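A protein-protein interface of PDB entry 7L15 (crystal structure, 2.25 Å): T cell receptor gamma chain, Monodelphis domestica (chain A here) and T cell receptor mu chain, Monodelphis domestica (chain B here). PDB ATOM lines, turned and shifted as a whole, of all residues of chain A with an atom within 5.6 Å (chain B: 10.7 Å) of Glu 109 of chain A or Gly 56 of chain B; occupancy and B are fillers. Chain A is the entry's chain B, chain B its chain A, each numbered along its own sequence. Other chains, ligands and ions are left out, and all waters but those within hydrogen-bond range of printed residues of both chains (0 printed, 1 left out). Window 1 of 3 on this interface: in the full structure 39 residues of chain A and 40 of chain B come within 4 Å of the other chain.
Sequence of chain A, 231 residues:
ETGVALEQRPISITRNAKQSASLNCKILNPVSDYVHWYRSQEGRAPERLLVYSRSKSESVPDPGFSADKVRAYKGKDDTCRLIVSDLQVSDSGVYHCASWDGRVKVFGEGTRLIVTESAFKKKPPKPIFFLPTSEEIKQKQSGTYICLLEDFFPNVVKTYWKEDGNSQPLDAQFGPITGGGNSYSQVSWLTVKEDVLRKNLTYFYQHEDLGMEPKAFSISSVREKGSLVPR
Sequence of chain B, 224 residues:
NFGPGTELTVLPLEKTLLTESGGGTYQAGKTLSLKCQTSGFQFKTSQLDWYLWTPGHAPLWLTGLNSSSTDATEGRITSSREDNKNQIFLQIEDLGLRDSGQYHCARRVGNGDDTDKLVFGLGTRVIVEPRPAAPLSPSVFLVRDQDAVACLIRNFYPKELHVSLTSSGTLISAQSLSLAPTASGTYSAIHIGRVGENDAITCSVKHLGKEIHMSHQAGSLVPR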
ATOM      1  N   LEU A   6      11.093   9.076 -29.772  1.00  0.00           N
ATOM      2  CA  LEU A   6      10.435   7.787 -29.910  1.00  0.00           C
ATOM      3  C   LEU A   6       8.972   7.997 -30.266  1.00  0.00           C
ATOM      4  O   LEU A   6       8.296   8.848 -29.679  1.00  0.00           O
ATOM      5  CB  LEU A   6      10.535   6.967 -28.619  1.00  0.00           C
ATOM      6  CG  LEU A   6      11.882   6.838 -27.900  1.00  0.00           C
ATOM      7  CD1 LEU A   6      12.221   8.110 -27.129  1.00  0.00           C
ATOM      8  CD2 LEU A   6      11.840   5.643 -26.965  1.00  0.00           C
ATOM      9  N   GLN A   8       5.115   6.152 -31.052  1.00  0.00           N
ATOM     10  CA  GLN A   8       4.292   5.004 -30.686  1.00  0.00           C
ATOM     11  C   GLN A   8       2.925   5.143 -31.334  1.00  0.00           C
ATOM     12  O   GLN A   8       2.232   6.139 -31.116  1.00  0.00           O
ATOM     13  CB  GLN A   8       4.143   4.879 -29.164  1.00  0.00           C
ATOM     14  CG  GLN A   8       5.426   4.494 -28.446  1.00  0.00           C
ATOM     15  CD  GLN A   8       5.203   4.203 -26.956  1.00  0.00           C
ATOM     16  OE1 GLN A   8       5.550   5.021 -26.091  1.00  0.00           O
ATOM     17  NE2 GLN A   8       4.644   3.031 -26.654  1.00  0.00           N
ATOM     18  N   VAL A  94      -1.127   2.327 -19.674  1.00  0.00           N
ATOM     19  CA  VAL A  94      -0.355   3.005 -20.713  1.00  0.00           C
ATOM     20  C   VAL A  94       1.062   2.453 -20.734  1.00  0.00           C
ATOM     21  O   VAL A  94       1.749   2.420 -19.700  1.00  0.00           O
ATOM     22  CB  VAL A  94      -0.360   4.527 -20.514  1.00  0.00           C
ATOM     23  CG1 VAL A  94       0.299   5.228 -21.712  1.00  0.00           C
ATOM     24  CG2 VAL A  94      -1.780   5.016 -20.328  1.00  0.00           C
ATOM     25  N   TYR A  95       1.501   2.026 -21.917  1.00  0.00           N
ATOM     26  CA  TYR A  95       2.811   1.424 -22.121  1.00  0.00           C
ATOM     27  C   TYR A  95       3.690   2.400 -22.892  1.00  0.00           C
ATOM     28  O   TYR A  95       3.352   2.797 -24.015  1.00  0.00           O
ATOM     29  CB  TYR A  95       2.681   0.104 -22.874  1.00  0.00           C
ATOM     30  CG  TYR A  95       2.007  -0.993 -22.084  1.00  0.00           C
ATOM     31  CD1 TYR A  95       0.677  -0.884 -21.706  1.00  0.00           C
ATOM     32  CD2 TYR A  95       2.702  -2.148 -21.722  1.00  0.00           C
ATOM     33  CE1 TYR A  95       0.055  -1.876 -20.987  1.00  0.00           C
ATOM     34  CE2 TYR A  95       2.080  -3.146 -20.983  1.00  0.00           C
ATOM     35  CZ  TYR A  95       0.750  -2.995 -20.618  1.00  0.00           C
ATOM     36  OH  TYR A  95       0.084  -3.967 -19.895  1.00  0.00           O
ATOM     37  N   HIS A  96       4.814   2.777 -22.298  1.00  0.00           N
ATOM     38  CA  HIS A  96       5.747   3.722 -22.887  1.00  0.00           C
ATOM     39  C   HIS A  96       7.043   3.004 -23.215  1.00  0.00           C
ATOM     40  O   HIS A  96       7.594   2.299 -22.363  1.00  0.00           O
ATOM     41  CB  HIS A  96       6.064   4.867 -21.928  1.00  0.00           C
ATOM     42  CG  HIS A  96       4.873   5.675 -21.508  1.00  0.00           C
ATOM     43  ND1 HIS A  96       4.523   6.851 -22.126  1.00  0.00           N
ATOM     44  CD2 HIS A  96       3.988   5.503 -20.499  1.00  0.00           C
ATOM     45  CE1 HIS A  96       3.460   7.360 -21.533  1.00  0.00           C
ATOM     46  NE2 HIS A  96       3.108   6.554 -20.549  1.00  0.00           N
ATOM     47  N   PHE A 107      11.158   9.327 -23.201  1.00  0.00           N
ATOM     48  CA  PHE A 107      10.027   8.413 -23.263  1.00  0.00           C
ATOM     49  C   PHE A 107       9.163   8.711 -24.474  1.00  0.00           C
ATOM     50  O   PHE A 107       8.928   9.875 -24.820  1.00  0.00           O
ATOM     51  CB  PHE A 107       9.125   8.529 -22.015  1.00  0.00           C
ATOM     52  CG  PHE A 107       9.695   7.900 -20.783  1.00  0.00           C
ATOM     53  CD1 PHE A 107      10.786   8.462 -20.135  1.00  0.00           C
ATOM     54  CD2 PHE A 107       9.115   6.748 -20.255  1.00  0.00           C
ATOM     55  CE1 PHE A 107      11.299   7.882 -18.991  1.00  0.00           C
ATOM     56  CE2 PHE A 107       9.616   6.162 -19.114  1.00  0.00           C
ATOM     57  CZ  PHE A 107      10.716   6.728 -18.476  1.00  0.00           C
ATOM     58  N   GLY A 108       8.650   7.656 -25.084  1.00  0.00           N
ATOM     59  CA  GLY A 108       7.573   7.811 -26.029  1.00  0.00           C
ATOM     60  C   GLY A 108       6.311   8.318 -25.357  1.00  0.00           C
ATOM     61  O   GLY A 108       6.159   8.344 -24.133  1.00  0.00           O
ATOM     62  N   GLU A 109       5.368   8.706 -26.206  1.00  0.00           N
ATOM     63  CA  GLU A 109       4.102   9.241 -25.746  1.00  0.00           C
ATOM     64  C   GLU A 109       3.183   8.158 -25.178  1.00  0.00           C
ATOM     65  O   GLU A 109       2.226   8.486 -24.488  1.00  0.00           O
ATOM     66  CB  GLU A 109       3.437   9.986 -26.920  1.00  0.00           C
ATOM     67  CG  GLU A 109       2.700  11.256 -26.539  1.00  0.00           C
ATOM     68  CD  GLU A 109       2.146  11.989 -27.756  1.00  0.00           C
ATOM     69  OE1 GLU A 109       1.091  11.558 -28.275  1.00  0.00           O
ATOM     70  OE2 GLU A 109       2.774  12.978 -28.203  1.00  0.00           O
ATOM     71  N   GLY A 110       3.435   6.886 -25.463  1.00  0.00           N
ATOM     72  CA  GLY A 110       2.646   5.819 -24.884  1.00  0.00           C
ATOM     73  C   GLY A 110       1.489   5.333 -25.732  1.00  0.00           C
ATOM     74  O   GLY A 110       0.839   6.124 -26.418  1.00  0.00           O
ATOM     75  N   THR A 111       1.231   4.028 -25.702  1.00  0.00           N
ATOM     76  CA  THR A 111       0.026   3.456 -26.275  1.00  0.00           C
ATOM     77  C   THR A 111      -0.823   2.876 -25.152  1.00  0.00           C
ATOM     78  O   THR A 111      -0.301   2.219 -24.244  1.00  0.00           O
ATOM     79  CB  THR A 111       0.366   2.374 -27.301  1.00  0.00           C
ATOM     80  OG1 THR A 111       1.054   2.962 -28.411  1.00  0.00           O
ATOM     81  CG2 THR A 111      -0.894   1.738 -27.834  1.00  0.00           C
ATOM     82  N   LYS A 158      -6.537  11.616 -30.256  1.00  0.00           N
ATOM     83  CA  LYS A 158      -5.515  12.649 -30.272  1.00  0.00           C
ATOM     84  C   LYS A 158      -5.829  13.589 -31.427  1.00  0.00           C
ATOM     85  O   LYS A 158      -6.066  13.130 -32.549  1.00  0.00           O
ATOM     86  CB  LYS A 158      -4.124  12.023 -30.425  1.00  0.00           C
ATOM     87  CG  LYS A 158      -2.972  13.006 -30.572  1.00  0.00           C
ATOM     88  CD  LYS A 158      -1.620  12.277 -30.597  1.00  0.00           C
ATOM     89  CE  LYS A 158      -0.432  13.240 -30.715  1.00  0.00           C
ATOM     90  NZ  LYS A 158       0.854  12.500 -30.929  1.00  0.00           N
ATOM     91  N   LEU B  52       7.977  14.429 -14.943  1.00  0.00           N
ATOM     92  CA  LEU B  52       6.599  14.885 -15.107  1.00  0.00           C
ATOM     93  C   LEU B  52       5.834  13.939 -16.032  1.00  0.00           C
ATOM     94  O   LEU B  52       6.159  13.825 -17.219  1.00  0.00           O
ATOM     95  CB  LEU B  52       6.563  16.307 -15.674  1.00  0.00           C
ATOM     96  CG  LEU B  52       5.136  16.830 -15.914  1.00  0.00           C
ATOM     97  CD1 LEU B  52       4.284  16.742 -14.626  1.00  0.00           C
ATOM     98  CD2 LEU B  52       5.134  18.257 -16.475  1.00  0.00           C
ATOM     99  N   TRP B  53       4.808  13.281 -15.498  1.00  0.00           N
ATOM    100  CA  TRP B  53       3.937  12.383 -16.258  1.00  0.00           C
ATOM    101  C   TRP B  53       2.602  13.092 -16.444  1.00  0.00           C
ATOM    102  O   TRP B  53       1.734  13.033 -15.575  1.00  0.00           O
ATOM    103  CB  TRP B  53       3.738  11.032 -15.544  1.00  0.00           C
ATOM    104  CG  TRP B  53       4.956  10.176 -15.528  1.00  0.00           C
ATOM    105  CD1 TRP B  53       6.152  10.458 -14.939  1.00  0.00           C
ATOM    106  CD2 TRP B  53       5.092   8.880 -16.112  1.00  0.00           C
ATOM    107  NE1 TRP B  53       7.034   9.415 -15.125  1.00  0.00           N
ATOM    108  CE2 TRP B  53       6.401   8.433 -15.841  1.00  0.00           C
ATOM    109  CE3 TRP B  53       4.232   8.054 -16.835  1.00  0.00           C
ATOM    110  CZ2 TRP B  53       6.869   7.213 -16.276  1.00  0.00           C
ATOM    111  CZ3 TRP B  53       4.689   6.845 -17.260  1.00  0.00           C
ATOM    112  CH2 TRP B  53       6.003   6.430 -16.985  1.00  0.00           C
ATOM    113  N   THR B  54       2.446  13.789 -17.570  1.00  0.00           N
ATOM    114  CA  THR B  54       1.134  14.388 -17.788  1.00  0.00           C
ATOM    115  C   THR B  54       0.303  13.462 -18.664  1.00  0.00           C
ATOM    116  O   THR B  54       0.766  13.066 -19.737  1.00  0.00           O
ATOM    117  CB  THR B  54       1.254  15.753 -18.450  1.00  0.00           C
ATOM    118  OG1 THR B  54       2.055  16.620 -17.644  1.00  0.00           O
ATOM    119  CG2 THR B  54      -0.114  16.374 -18.612  1.00  0.00           C
ATOM    120  N   PRO B  55      -0.920  13.114 -18.271  1.00  0.00           N
ATOM    121  CA  PRO B  55      -1.707  12.183 -19.085  1.00  0.00           C
ATOM    122  C   PRO B  55      -1.783  12.662 -20.524  1.00  0.00           C
ATOM    123  O   PRO B  55      -1.975  13.846 -20.792  1.00  0.00           O
ATOM    124  CB  PRO B  55      -3.072  12.183 -18.393  1.00  0.00           C
ATOM    125  CG  PRO B  55      -2.722  12.449 -16.938  1.00  0.00           C
ATOM    126  CD  PRO B  55      -1.597  13.451 -17.004  1.00  0.00           C
ATOM    127  N   GLY B  56      -1.545  11.739 -21.454  1.00  0.00           N
ATOM    128  CA  GLY B  56      -1.552  12.047 -22.865  1.00  0.00           C
ATOM    129  C   GLY B  56      -0.233  12.527 -23.433  1.00  0.00           C
ATOM    130  O   GLY B  56      -0.130  12.691 -24.654  1.00  0.00           O
ATOM    131  N   HIS B  57       0.780  12.760 -22.597  1.00  0.00           N
ATOM    132  CA  HIS B  57       2.069  13.248 -23.065  1.00  0.00           C
ATOM    133  C   HIS B  57       3.154  12.231 -22.739  1.00  0.00           C
ATOM    134  O   HIS B  57       2.960  11.308 -21.943  1.00  0.00           O
ATOM    135  CB  HIS B  57       2.435  14.605 -22.438  1.00  0.00           C
ATOM    136  CG  HIS B  57       1.578  15.746 -22.887  1.00  0.00           C
ATOM    137  ND1 HIS B  57       0.327  15.993 -22.359  1.00  0.00           N
ATOM    138  CD2 HIS B  57       1.798  16.719 -23.802  1.00  0.00           C
ATOM    139  CE1 HIS B  57      -0.188  17.063 -22.937  1.00  0.00           C
ATOM    140  NE2 HIS B  57       0.685  17.523 -23.816  1.00  0.00           N
ATOM    141  N   ALA B  58       4.314  12.437 -23.352  1.00  0.00           N
ATOM    142  CA  ALA B  58       5.504  11.676 -22.991  1.00  0.00           C
ATOM    143  C   ALA B  58       5.967  12.072 -21.594  1.00  0.00           C
ATOM    144  O   ALA B  58       6.017  13.269 -21.282  1.00  0.00           O
ATOM    145  CB  ALA B  58       6.620  11.924 -24.007  1.00  0.00           C
ATOM    146  N   PRO B  59       6.277  11.111 -20.723  1.00  0.00           N
ATOM    147  CA  PRO B  59       6.923  11.449 -19.456  1.00  0.00           C
ATOM    148  C   PRO B  59       8.177  12.256 -19.742  1.00  0.00           C
ATOM    149  O   PRO B  59       8.922  11.957 -20.675  1.00  0.00           O
ATOM    150  CB  PRO B  59       7.259  10.084 -18.848  1.00  0.00           C
ATOM    151  CG  PRO B  59       6.293   9.144 -19.446  1.00  0.00           C
ATOM    152  CD  PRO B  59       5.916   9.691 -20.810  1.00  0.00           C
ATOM    153  N   LEU B  60       8.411  13.290 -18.942  1.00  0.00           N
ATOM    154  CA  LEU B  60       9.461  14.239 -19.262  1.00  0.00           C
ATOM    155  C   LEU B  60      10.403  14.395 -18.077  1.00  0.00           C
ATOM    156  O   LEU B  60       9.966  14.651 -16.953  1.00  0.00           O
ATOM    157  CB  LEU B  60       8.849  15.593 -19.655  1.00  0.00           C
ATOM    158  CG  LEU B  60       9.740  16.648 -20.320  1.00  0.00           C
ATOM    159  CD1 LEU B  60      10.426  16.109 -21.574  1.00  0.00           C
ATOM    160  CD2 LEU B  60       8.883  17.872 -20.631  1.00  0.00           C
ATOM    161  N   SER B 100       0.923  21.318 -15.252  1.00  0.00           N
ATOM    162  CA  SER B 100       0.004  20.377 -14.615  1.00  0.00           C
ATOM    163  C   SER B 100       0.364  18.931 -14.948  1.00  0.00           C
ATOM    164  O   SER B 100       0.818  18.616 -16.045  1.00  0.00           O
ATOM    165  CB  SER B 100      -1.442  20.637 -15.066  1.00  0.00           C
ATOM    166  OG  SER B 100      -1.888  21.914 -14.644  1.00  0.00           O
ATOM    167  N   GLY B 101       0.143  18.048 -13.996  1.00  0.00           N
ATOM    168  CA  GLY B 101       0.368  16.642 -14.230  1.00  0.00           C
ATOM    169  C   GLY B 101       0.768  15.943 -12.944  1.00  0.00           C
ATOM    170  O   GLY B 101       0.577  16.461 -11.847  1.00  0.00           O
ATOM    171  N   GLN B 102       1.308  14.744 -13.111  1.00  0.00           N
ATOM    172  CA  GLN B 102       1.715  13.908 -11.995  1.00  0.00           C
ATOM    173  C   GLN B 102       3.235  13.960 -11.877  1.00  0.00           C
ATOM    174  O   GLN B 102       3.946  13.491 -12.771  1.00  0.00           O
ATOM    175  CB  GLN B 102       1.241  12.473 -12.202  1.00  0.00           C
ATOM    176  CG  GLN B 102       1.453  11.594 -10.987  1.00  0.00           C
ATOM    177  CD  GLN B 102       0.305  11.699  -9.995  1.00  0.00           C
ATOM    178  OE1 GLN B 102      -0.663  12.435 -10.223  1.00  0.00           O
ATOM    179  NE2 GLN B 102       0.398  10.941  -8.898  1.00  0.00           N
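The backbone NH (N) of Trp 53 of chain B lies within hydrogen-bond range of the backbone carbonyl oxygen (O) of Gln 102 of chain B (2.9 Å). ND1 of His 96 of chain A sits at hydrogen-bond distance from O of Gly 108 of chain A (3.0 Å). The side-chain carboxylate (OE1) of Glu 109 of chain A is in salt-bridge range of the side-chain amino group (NZ) of Lys 158 of chain A, at 2.8 Å.
Of the 11 printed residues of chain A, 4 touch a printed residue of chain B. Printed residues of chain A that touch a printed residue of chain B: His 96, Phe 107, Gly 108 and Glu 109. Along chain A the printed residues that touch a printed residue of chain B span positions 96 to 109. Among the printed residues, no Asp or Glu carboxylate lies within 4 Å of a Lys or Arg side-chain nitrogen of the other chain.
No residue of chain B comes within 4 Å of Gln 8 of chain A. Of the printed residues of chain B, His 96 of chain A touches Trp 53 (3.6 Å) and Pro 59 (3.4 Å). Of the printed residues of chain B, Phe 107 of chain A touches Ala 58 and Pro 59. No residue of chain B comes within 4 Å of Gly 110 of chain A. Gly 56 of chain B touches just one residue of chain A: Glu 109. Of the printed residues of chain A, His 57 of chain B touches Glu 109. Printed residues of chain A within 4 Å of Ala 58 of chain B: Phe 107 (3.2 Å), Gly 108 (3.6 Å) and Glu 109 (3.8 Å). Of the printed residues of chain A, Pro 59 of chain B touches His 96 (3.4 Å), Phe 107 (3.6 Å) and Gly 108 (3.6 Å). The nearest residue of chain B that does not touch Glu 109 of chain A is Pro 59 of chain B (5.3 Å). The nearest printed residue of chain A that does not touch Trp 53 of chain B is Phe 107 of chain A (4.1 Å).
His 96 of chain A touches Trp 53 of chain B (CD2 to CZ3, 3.6 Å). ND1 of His 96 of chain A touches CD of Pro 59 of chain B, at 3.4 Å. Ala 58 of chain B touches Phe 107 of chain A. CB of Phe 107 of chain A touches CD of Pro 59 of chain B, 3.6 Å away. Gly 108 of chain A touches Ala 58 of chain B. Pro 59 of chain B touches Gly 108 of chain A. CG of Glu 109 of chain A touches O of Gly 56 of chain B (3.7 Å). O of Glu 109 of chain A touches O of His 57 of chain B, 3.9 Å away. Glu 109 of chain A touches Ala 58 of chain B.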
